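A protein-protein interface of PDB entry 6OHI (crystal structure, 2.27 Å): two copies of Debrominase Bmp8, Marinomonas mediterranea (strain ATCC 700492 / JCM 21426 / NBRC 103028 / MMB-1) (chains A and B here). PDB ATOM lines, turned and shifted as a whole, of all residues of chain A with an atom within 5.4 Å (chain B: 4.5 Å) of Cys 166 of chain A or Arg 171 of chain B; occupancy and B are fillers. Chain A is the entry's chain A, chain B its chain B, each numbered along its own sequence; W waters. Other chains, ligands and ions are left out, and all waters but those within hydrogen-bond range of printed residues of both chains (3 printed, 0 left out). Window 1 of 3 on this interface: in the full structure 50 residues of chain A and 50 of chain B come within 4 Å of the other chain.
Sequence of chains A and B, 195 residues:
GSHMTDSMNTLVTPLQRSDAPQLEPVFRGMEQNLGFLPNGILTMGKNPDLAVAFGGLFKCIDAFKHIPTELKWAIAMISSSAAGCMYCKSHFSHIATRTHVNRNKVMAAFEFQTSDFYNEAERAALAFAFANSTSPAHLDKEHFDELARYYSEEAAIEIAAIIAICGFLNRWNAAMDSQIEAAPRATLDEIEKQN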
ATOM      1  N   ILE A  75     -26.875  -6.453   0.369  1.00  0.00           N
ATOM      2  CA  ILE A  75     -26.021  -5.923  -0.715  1.00  0.00           C
ATOM      3  C   ILE A  75     -24.794  -6.824  -0.905  1.00  0.00           C
ATOM      4  O   ILE A  75     -24.444  -7.170  -2.033  1.00  0.00           O
ATOM      5  CB  ILE A  75     -25.596  -4.470  -0.440  1.00  0.00           C
ATOM      6  CG1 ILE A  75     -26.761  -3.500  -0.613  1.00  0.00           C
ATOM      7  CG2 ILE A  75     -24.415  -4.068  -1.309  1.00  0.00           C
ATOM      8  CD1 ILE A  75     -26.544  -2.178   0.089  1.00  0.00           C
ATOM      9  N   ALA A  76     -24.135  -7.165   0.206  1.00  0.00           N
ATOM     10  CA  ALA A  76     -22.920  -7.962   0.186  1.00  0.00           C
ATOM     11  C   ALA A  76     -23.226  -9.379  -0.300  1.00  0.00           C
ATOM     12  O   ALA A  76     -22.419  -9.979  -0.979  1.00  0.00           O
ATOM     13  CB  ALA A  76     -22.299  -7.981   1.554  1.00  0.00           C
ATOM     14  N   SER A  79     -23.989  -8.906  -4.269  1.00  0.00           N
ATOM     15  CA  SER A  79     -22.723  -8.584  -4.917  1.00  0.00           C
ATOM     16  C   SER A  79     -21.845  -9.835  -5.038  1.00  0.00           C
ATOM     17  O   SER A  79     -21.306 -10.125  -6.105  1.00  0.00           O
ATOM     18  CB  SER A  79     -22.002  -7.491  -4.179  1.00  0.00           C
ATOM     19  OG  SER A  79     -20.672  -7.351  -4.648  1.00  0.00           O
ATOM     20  N   SER A  80     -21.695 -10.561  -3.927  1.00  0.00           N
ATOM     21  CA  SER A  80     -20.834 -11.735  -3.872  1.00  0.00           C
ATOM     22  C   SER A  80     -21.379 -12.818  -4.804  1.00  0.00           C
ATOM     23  O   SER A  80     -20.617 -13.536  -5.444  1.00  0.00           O
ATOM     24  CB  SER A  80     -20.693 -12.253  -2.461  1.00  0.00           C
ATOM     25  OG  SER A  80     -20.085 -11.283  -1.626  1.00  0.00           O
ATOM     26  N   ALA A  83     -20.814 -11.938  -8.434  1.00  0.00           N
ATOM     27  CA  ALA A  83     -19.402 -12.148  -8.740  1.00  0.00           C
ATOM     28  C   ALA A  83     -19.049 -13.639  -8.730  1.00  0.00           C
ATOM     29  O   ALA A  83     -17.931 -13.994  -9.054  1.00  0.00           O
ATOM     30  CB  ALA A  83     -18.540 -11.392  -7.769  1.00  0.00           C
ATOM     31  N   PHE A  92     -21.699 -13.849   3.939  1.00  0.00           N
ATOM     32  CA  PHE A  92     -22.584 -12.710   4.089  1.00  0.00           C
ATOM     33  C   PHE A  92     -24.016 -13.203   4.335  1.00  0.00           C
ATOM     34  O   PHE A  92     -24.773 -12.563   5.051  1.00  0.00           O
ATOM     35  CB  PHE A  92     -22.473 -11.790   2.875  1.00  0.00           C
ATOM     36  CG  PHE A  92     -21.166 -11.045   2.766  1.00  0.00           C
ATOM     37  CD1 PHE A  92     -20.709 -10.249   3.805  1.00  0.00           C
ATOM     38  CD2 PHE A  92     -20.406 -11.112   1.605  1.00  0.00           C
ATOM     39  CE1 PHE A  92     -19.516  -9.549   3.692  1.00  0.00           C
ATOM     40  CE2 PHE A  92     -19.210 -10.421   1.498  1.00  0.00           C
ATOM     41  CZ  PHE A  92     -18.771  -9.632   2.541  1.00  0.00           C
ATOM     42  N   ASN A 132     -23.201  -4.227 -10.624  1.00  0.00           N
ATOM     43  CA  ASN A 132     -21.930  -3.596 -10.303  1.00  0.00           C
ATOM     44  C   ASN A 132     -20.829  -4.660 -10.186  1.00  0.00           C
ATOM     45  O   ASN A 132     -19.642  -4.339 -10.343  1.00  0.00           O
ATOM     46  CB  ASN A 132     -22.084  -2.785  -9.013  1.00  0.00           C
ATOM     47  CG  ASN A 132     -20.969  -1.808  -8.704  1.00  0.00           C
ATOM     48  OD1 ASN A 132     -21.038  -1.132  -7.687  1.00  0.00           O
ATOM     49  ND2 ASN A 132     -19.952  -1.713  -9.545  1.00  0.00           N
ATOM     50  N   SER A 133     -21.220  -5.918  -9.923  1.00  0.00           N
ATOM     51  CA  SER A 133     -20.305  -6.932  -9.394  1.00  0.00           C
ATOM     52  C   SER A 133     -19.883  -7.968 -10.445  1.00  0.00           C
ATOM     53  O   SER A 133     -19.006  -8.800 -10.176  1.00  0.00           O
ATOM     54  CB  SER A 133     -20.917  -7.596  -8.201  1.00  0.00           C
ATOM     55  OG  SER A 133     -21.125  -6.658  -7.157  1.00  0.00           O
ATOM     56  N   ALA A 161     -19.774   1.532  -1.614  1.00  0.00           N
ATOM     57  CA  ALA A 161     -18.647   1.172  -0.751  1.00  0.00           C
ATOM     58  C   ALA A 161     -18.719  -0.305  -0.353  1.00  0.00           C
ATOM     59  O   ALA A 161     -17.698  -0.989  -0.348  1.00  0.00           O
ATOM     60  CB  ALA A 161     -18.620   2.058   0.471  1.00  0.00           C
ATOM     61  N   ILE A 162     -19.920  -0.787  -0.009  1.00  0.00           N
ATOM     62  CA  ILE A 162     -20.098  -2.178   0.413  1.00  0.00           C
ATOM     63  C   ILE A 162     -19.782  -3.096  -0.778  1.00  0.00           C
ATOM     64  O   ILE A 162     -19.062  -4.072  -0.645  1.00  0.00           O
ATOM     65  CB  ILE A 162     -21.511  -2.428   0.987  1.00  0.00           C
ATOM     66  CG1 ILE A 162     -21.733  -1.693   2.312  1.00  0.00           C
ATOM     67  CG2 ILE A 162     -21.768  -3.919   1.134  1.00  0.00           C
ATOM     68  CD1 ILE A 162     -23.180  -1.661   2.763  1.00  0.00           C
ATOM     69  N   ILE A 163     -20.314  -2.744  -1.949  1.00  0.00           N
ATOM     70  CA  ILE A 163     -20.069  -3.498  -3.159  1.00  0.00           C
ATOM     71  C   ILE A 163     -18.556  -3.548  -3.407  1.00  0.00           C
ATOM     72  O   ILE A 163     -18.018  -4.599  -3.700  1.00  0.00           O
ATOM     73  CB  ILE A 163     -20.830  -2.890  -4.349  1.00  0.00           C
ATOM     74  CG1 ILE A 163     -22.346  -2.958  -4.150  1.00  0.00           C
ATOM     75  CG2 ILE A 163     -20.406  -3.559  -5.642  1.00  0.00           C
ATOM     76  CD1 ILE A 163     -23.115  -1.965  -4.993  1.00  0.00           C
ATOM     77  N   ALA A 164     -17.883  -2.405  -3.270  1.00  0.00           N
ATOM     78  CA  ALA A 164     -16.462  -2.301  -3.580  1.00  0.00           C
ATOM     79  C   ALA A 164     -15.650  -3.145  -2.593  1.00  0.00           C
ATOM     80  O   ALA A 164     -14.713  -3.837  -2.993  1.00  0.00           O
ATOM     81  CB  ALA A 164     -16.027  -0.852  -3.584  1.00  0.00           C
ATOM     82  N   ILE A 165     -16.038  -3.121  -1.312  1.00  0.00           N
ATOM     83  CA  ILE A 165     -15.384  -3.934  -0.284  1.00  0.00           C
ATOM     84  C   ILE A 165     -15.570  -5.423  -0.612  1.00  0.00           C
ATOM     85  O   ILE A 165     -14.666  -6.224  -0.382  1.00  0.00           O
ATOM     86  CB  ILE A 165     -15.895  -3.570   1.123  1.00  0.00           C
ATOM     87  CG1 ILE A 165     -15.435  -2.169   1.533  1.00  0.00           C
ATOM     88  CG2 ILE A 165     -15.464  -4.611   2.138  1.00  0.00           C
ATOM     89  CD1 ILE A 165     -16.184  -1.596   2.713  1.00  0.00           C
ATOM     90  N   CYS A 166     -16.738  -5.791  -1.149  1.00  0.00           N
ATOM     91  CA  CYS A 166     -16.959  -7.149  -1.617  1.00  0.00           C
ATOM     92  C   CYS A 166     -16.022  -7.461  -2.786  1.00  0.00           C
ATOM     93  O   CYS A 166     -15.561  -8.593  -2.917  1.00  0.00           O
ATOM     94  CB  CYS A 166     -18.402  -7.373  -2.041  1.00  0.00           C
ATOM     95  SG  CYS A 166     -19.539  -7.388  -0.638  1.00  0.00           S
ATOM     96  N   GLY A 167     -15.766  -6.453  -3.630  1.00  0.00           N
ATOM     97  CA  GLY A 167     -14.763  -6.552  -4.666  1.00  0.00           C
ATOM     98  C   GLY A 167     -13.468  -7.104  -4.109  1.00  0.00           C
ATOM     99  O   GLY A 167     -12.897  -8.052  -4.648  1.00  0.00           O
ATOM    100  N   PHE A 168     -13.013  -6.505  -3.009  1.00  0.00           N
ATOM    101  CA  PHE A 168     -11.779  -6.920  -2.378  1.00  0.00           C
ATOM    102  C   PHE A 168     -11.916  -8.367  -1.882  1.00  0.00           C
ATOM    103  O   PHE A 168     -11.065  -9.203  -2.166  1.00  0.00           O
ATOM    104  CB  PHE A 168     -11.394  -5.949  -1.260  1.00  0.00           C
ATOM    105  CG  PHE A 168     -10.101  -6.306  -0.573  1.00  0.00           C
ATOM    106  CD1 PHE A 168     -10.066  -7.300   0.390  1.00  0.00           C
ATOM    107  CD2 PHE A 168      -8.920  -5.686  -0.919  1.00  0.00           C
ATOM    108  CE1 PHE A 168      -8.877  -7.662   1.001  1.00  0.00           C
ATOM    109  CE2 PHE A 168      -7.727  -6.042  -0.304  1.00  0.00           C
ATOM    110  CZ  PHE A 168      -7.703  -7.030   0.653  1.00  0.00           C
ATOM    111  N   LEU A 169     -12.991  -8.657  -1.139  1.00  0.00           N
ATOM    112  CA  LEU A 169     -13.107  -9.940  -0.437  1.00  0.00           C
ATOM    113  C   LEU A 169     -13.389 -11.093  -1.408  1.00  0.00           C
ATOM    114  O   LEU A 169     -12.939 -12.213  -1.155  1.00  0.00           O
ATOM    115  CB  LEU A 169     -14.197  -9.858   0.634  1.00  0.00           C
ATOM    116  CG  LEU A 169     -13.749  -9.234   1.951  1.00  0.00           C
ATOM    117  CD1 LEU A 169     -14.915  -9.115   2.929  1.00  0.00           C
ATOM    118  CD2 LEU A 169     -12.611 -10.039   2.565  1.00  0.00           C
ATOM    119  N   ASN A 170     -14.146 -10.826  -2.482  1.00  0.00           N
ATOM    120  CA  ASN A 170     -14.470 -11.853  -3.486  1.00  0.00           C
ATOM    121  C   ASN A 170     -13.165 -12.342  -4.129  1.00  0.00           C
ATOM    122  O   ASN A 170     -12.971 -13.540  -4.285  1.00  0.00           O
ATOM    123  CB  ASN A 170     -15.416 -11.348  -4.576  1.00  0.00           C
ATOM    124  CG  ASN A 170     -16.787 -10.947  -4.076  1.00  0.00           C
ATOM    125  OD1 ASN A 170     -17.509 -10.226  -4.765  1.00  0.00           O
ATOM    126  ND2 ASN A 170     -17.164 -11.416  -2.898  1.00  0.00           N
ATOM    127  N   ARG A 171     -12.289 -11.392  -4.488  1.00  0.00           N
ATOM    128  CA  ARG A 171     -11.039 -11.684  -5.157  1.00  0.00           C
ATOM    129  C   ARG A 171     -10.048 -12.294  -4.161  1.00  0.00           C
ATOM    130  O   ARG A 171      -9.381 -13.285  -4.474  1.00  0.00           O
ATOM    131  CB  ARG A 171     -10.488 -10.428  -5.836  1.00  0.00           C
ATOM    132  CG  ARG A 171     -11.381  -9.926  -6.962  1.00  0.00           C
ATOM    133  CD  ARG A 171     -10.669  -9.059  -7.971  1.00  0.00           C
ATOM    134  NE  ARG A 171     -11.623  -8.419  -8.857  1.00  0.00           N
ATOM    135  CZ  ARG A 171     -11.319  -7.407  -9.663  1.00  0.00           C
ATOM    136  NH1 ARG A 171     -10.060  -6.992  -9.767  1.00  0.00           N
ATOM    137  NH2 ARG A 171     -12.282  -6.806 -10.333  1.00  0.00           N
ATOM    138  N   GLY B 167     -10.144  -5.092  -7.154  1.00  0.00           N
ATOM    139  CA  GLY B 167     -11.517  -5.473  -6.869  1.00  0.00           C
ATOM    140  C   GLY B 167     -12.316  -4.280  -6.381  1.00  0.00           C
ATOM    141  O   GLY B 167     -13.397  -3.990  -6.893  1.00  0.00           O
ATOM    142  N   PHE B 168     -11.755  -3.575  -5.397  1.00  0.00           N
ATOM    143  CA  PHE B 168     -12.387  -2.403  -4.833  1.00  0.00           C
ATOM    144  C   PHE B 168     -12.548  -1.331  -5.920  1.00  0.00           C
ATOM    145  O   PHE B 168     -13.644  -0.810  -6.133  1.00  0.00           O
ATOM    146  CB  PHE B 168     -11.599  -1.879  -3.624  1.00  0.00           C
ATOM    147  CG  PHE B 168     -12.277  -0.719  -2.949  1.00  0.00           C
ATOM    148  CD1 PHE B 168     -12.194   0.565  -3.475  1.00  0.00           C
ATOM    149  CD2 PHE B 168     -13.049  -0.923  -1.819  1.00  0.00           C
ATOM    150  CE1 PHE B 168     -12.859   1.624  -2.874  1.00  0.00           C
ATOM    151  CE2 PHE B 168     -13.709   0.138  -1.221  1.00  0.00           C
ATOM    152  CZ  PHE B 168     -13.618   1.405  -1.751  1.00  0.00           C
ATOM    153  N   LEU B 169     -11.453  -1.009  -6.612  1.00  0.00           N
ATOM    154  CA  LEU B 169     -11.430   0.150  -7.510  1.00  0.00           C
ATOM    155  C   LEU B 169     -12.231  -0.112  -8.789  1.00  0.00           C
ATOM    156  O   LEU B 169     -12.820   0.819  -9.330  1.00  0.00           O
ATOM    157  CB  LEU B 169      -9.985   0.517  -7.844  1.00  0.00           C
ATOM    158  CG  LEU B 169      -9.296   1.378  -6.791  1.00  0.00           C
ATOM    159  CD1 LEU B 169      -7.829   1.570  -7.138  1.00  0.00           C
ATOM    160  CD2 LEU B 169      -9.986   2.719  -6.648  1.00  0.00           C
ATOM    161  N   ASN B 170     -12.221  -1.355  -9.281  1.00  0.00           N
ATOM    162  CA  ASN B 170     -12.974  -1.726 -10.483  1.00  0.00           C
ATOM    163  C   ASN B 170     -14.471  -1.490 -10.235  1.00  0.00           C
ATOM    164  O   ASN B 170     -15.159  -0.920 -11.097  1.00  0.00           O
ATOM    165  CB  ASN B 170     -12.748  -3.182 -10.908  1.00  0.00           C
ATOM    166  CG  ASN B 170     -11.327  -3.496 -11.318  1.00  0.00           C
ATOM    167  OD1 ASN B 170     -10.949  -4.661 -11.355  1.00  0.00           O
ATOM    168  ND2 ASN B 170     -10.531  -2.483 -11.624  1.00  0.00           N
ATOM    169  N   ARG B 171     -14.958  -1.934  -9.066  1.00  0.00           N
ATOM    170  CA  ARG B 171     -16.371  -1.834  -8.711  1.00  0.00           C
ATOM    171  C   ARG B 171     -16.712  -0.379  -8.372  1.00  0.00           C
ATOM    172  O   ARG B 171     -17.747   0.134  -8.822  1.00  0.00           O
ATOM    173  CB  ARG B 171     -16.712  -2.803  -7.572  1.00  0.00           C
ATOM    174  CG  ARG B 171     -16.560  -4.264  -7.974  1.00  0.00           C
ATOM    175  CD  ARG B 171     -17.309  -5.257  -7.111  1.00  0.00           C
ATOM    176  NE  ARG B 171     -16.857  -6.605  -7.441  1.00  0.00           N
ATOM    177  CZ  ARG B 171     -17.171  -7.696  -6.756  1.00  0.00           C
ATOM    178  NH1 ARG B 171     -18.020  -7.616  -5.742  1.00  0.00           N
ATOM    179  NH2 ARG B 171     -16.638  -8.857  -7.084  1.00  0.00           N
ATOM    180  N   TRP B 172     -15.835   0.278  -7.603  1.00  0.00           N
ATOM    181  CA  TRP B 172     -16.045   1.673  -7.206  1.00  0.00           C
ATOM    182  C   TRP B 172     -16.197   2.570  -8.443  1.00  0.00           C
ATOM    183  O   TRP B 172     -17.136   3.365  -8.528  1.00  0.00           O
ATOM    184  CB  TRP B 172     -14.924   2.182  -6.291  1.00  0.00           C
ATOM    185  CG  TRP B 172     -15.141   3.613  -5.905  1.00  0.00           C
ATOM    186  CD1 TRP B 172     -14.566   4.712  -6.473  1.00  0.00           C
ATOM    187  CD2 TRP B 172     -16.060   4.107  -4.916  1.00  0.00           C
ATOM    188  NE1 TRP B 172     -15.052   5.853  -5.898  1.00  0.00           N
ATOM    189  CE2 TRP B 172     -15.959   5.513  -4.929  1.00  0.00           C
ATOM    190  CE3 TRP B 172     -16.924   3.504  -3.999  1.00  0.00           C
ATOM    191  CZ2 TRP B 172     -16.714   6.319  -4.082  1.00  0.00           C
ATOM    192  CZ3 TRP B 172     -17.664   4.303  -3.154  1.00  0.00           C
ATOM    193  CH2 TRP B 172     -17.561   5.694  -3.198  1.00  0.00           C
ATOM    194  N   ASN B 173     -15.287   2.430  -9.413  1.00  0.00           N
ATOM    195  CA  ASN B 173     -15.280   3.303 -10.585  1.00  0.00           C
ATOM    196  C   ASN B 173     -16.425   2.945 -11.541  1.00  0.00           C
ATOM    197  O   ASN B 173     -16.862   3.791 -12.311  1.00  0.00           O
ATOM    198  CB  ASN B 173     -13.922   3.291 -11.281  1.00  0.00           C
ATOM    199  CG  ASN B 173     -12.912   4.106 -10.510  1.00  0.00           C
ATOM    200  OD1 ASN B 173     -13.166   5.277 -10.215  1.00  0.00           O
ATOM    201  ND2 ASN B 173     -11.782   3.497 -10.181  1.00  0.00           N
ATOM    202  N   ALA B 174     -16.900   1.698 -11.490  1.00  0.00           N
ATOM    203  CA  ALA B 174     -18.103   1.316 -12.212  1.00  0.00           C
ATOM    204  C   ALA B 174     -19.334   1.953 -11.545  1.00  0.00           C
ATOM    205  O   ALA B 174     -20.241   2.422 -12.233  1.00  0.00           O
ATOM    206  CB  ALA B 174     -18.212  -0.189 -12.278  1.00  0.00           C
ATOM    207  N   ALA B 175     -19.346   1.981 -10.206  1.00  0.00           N
ATOM    208  CA  ALA B 175     -20.476   2.530  -9.434  1.00  0.00           C
ATOM    209  C   ALA B 175     -20.588   4.057  -9.599  1.00  0.00           C
ATOM    210  O   ALA B 175     -21.678   4.598  -9.544  1.00  0.00           O
ATOM    211  CB  ALA B 175     -20.337   2.139  -7.981  1.00  0.00           C
HETATM  212  O   HOH W   1     -18.784  -0.249  -6.086  1.00  0.00           O
HETATM  213  O   HOH W   2     -15.348  -6.661 -10.068  1.00  0.00           O
HETATM  214  O   HOH W   3     -14.295  -9.620  -8.631  1.00  0.00           O
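The side-chain hydroxyl (OG) of Ser 79 of chain A is in hydrogen-bond range of the guanidinium group (NH1) of Arg 171 of chain B, 2.9 Å away. The backbone carbonyl oxygen (O) of Arg 171 of chain B lies within hydrogen-bond range of the side-chain amide nitrogen (ND2) of Asn 132 of chain A. The guanidinium group (NH2) of Arg 171 of chain B is in hydrogen-bond range of the side-chain amide oxygen (OD1) of Asn 170 of chain A. The guanidinium group (NH2) of Arg 171 of chain A sits at hydrogen-bond distance from the side-chain amide oxygen (OD1) of Asn 170 of chain B. The backbone NH (N) of Gly 167 of chain A sits close to the guanidinium group (NH1) of Arg 171 of chain B. NH1 of Arg 171 of chain A sits close to N of Gly 167 of chain B, at 3.2 Å.
The side-chain hydroxyl of Ser 79 of chain A is in hydrogen-bond range of the side-chain hydroxyl of Ser 133 of chain A, 2.6 Å away. The side-chain hydroxyl (OG) of Ser 80 of chain A sits at hydrogen-bond distance from the side-chain amide nitrogen (ND2) of Asn 170 of chain A, 3.2 Å away. O of Ile 162 of chain A sits at hydrogen-bond distance from SG of Cys 166 of chain A. The side-chain amide oxygen (OD1) of Asn 170 of chain A lies close to the backbone carbonyl oxygen (O) of Cys 166 of chain A (3.1 Å).
Ala 174 of chain B touches Asn 132 of chain A (CB to ND2, 3.6 Å). Asn 132 of chain A touches Ala 175 of chain B (OD1 to CB, 3.4 Å). Arg 171 of chain B touches Ser 133 of chain A. Ala 161 of chain A touches Trp 172 of chain B. O of Ile 163 of chain A touches CD of Arg 171 of chain B, at 3.5 Å. Phe 168 of chain B touches Ala 164 of chain A (CA to O, 3.3 Å). Ile 165 of chain A touches Phe 168 of chain B (N to CD2, 3.7 Å). Cys 166 of chain A touches Arg 171 of chain B. Gly 167 of chain A touches Gly 167 of chain B (CA to O, 3.7 Å). N of Phe 168 of chain A touches N of Phe 168 of chain B (3.98 Å).
Of the printed residues of chain B, Ser 79 of chain A touches Arg 171 (2.9 Å). Of the printed residues of chain B, Ile 163 of chain A touches Arg 171 (3.5 Å). Cys 166 of chain A touches just one residue of chain B: Arg 171 (3.6 Å). Of the printed residues of chain B, Asn 170 of chain A touches Arg 171 (2.8 Å). Of the printed residues of chain A, Gly 167 of chain B touches Gly 167 and Arg 171. The nearest residue of chain A that does not touch Arg 171 of chain B is Ala 164 of chain A (4.03 Å). The nearest printed residue of chain B that does not touch Ala 161 of chain A is Phe 168 of chain B (4.2 Å).
Printed residues of chain B that touch a printed residue of chain A: Gly 167, Phe 168, Asn 170, Arg 171, Trp 172, Ala 174 and Ala 175. Of the 19 printed residues of chain A, 13 touch a printed residue of chain B. Hydrophobic or aromatic side chains of chain A that line the printed part of chain B: Ala 83, Ile 163, Ala 164 and Ile 165.
Gly 167 of chain B touches its own counterpart, Gly 167 of chain A. Gly 167 of chain A touches Arg 171 of chain B, and with the chains exchanged Arg 171 of chain A touches Gly 167 of chain B. Phe 168 of chain A touches its own counterpart, Phe 168 of chain B. Asn 170 of chain A touches Arg 171 of chain B, and with the chains exchanged Arg 171 of chain A touches Asn 170 of chain B. Of the 17 pairs that touch across the chains among the printed residues, 6 have their exchanged pair printed and touching as well.
Water W1 lies within hydrogen-bond range of OD1 of Asn 132 of chain A (2.9 Å), O of Arg 171 of chain B (3.0 Å) and N of Trp 172 of chain B (3.4 Å). Water W3 bridges NH2 of Arg 171 of chain B (2.9 Å) and NE of Arg 171 of chain A (2.9 Å). Water W2 lies within hydrogen-bond range of the guanidinium group (NE) of Arg 171 of chain B (3.0 Å) and the guanidinium group (NH2) of Arg 171 of chain A (3.1 Å).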
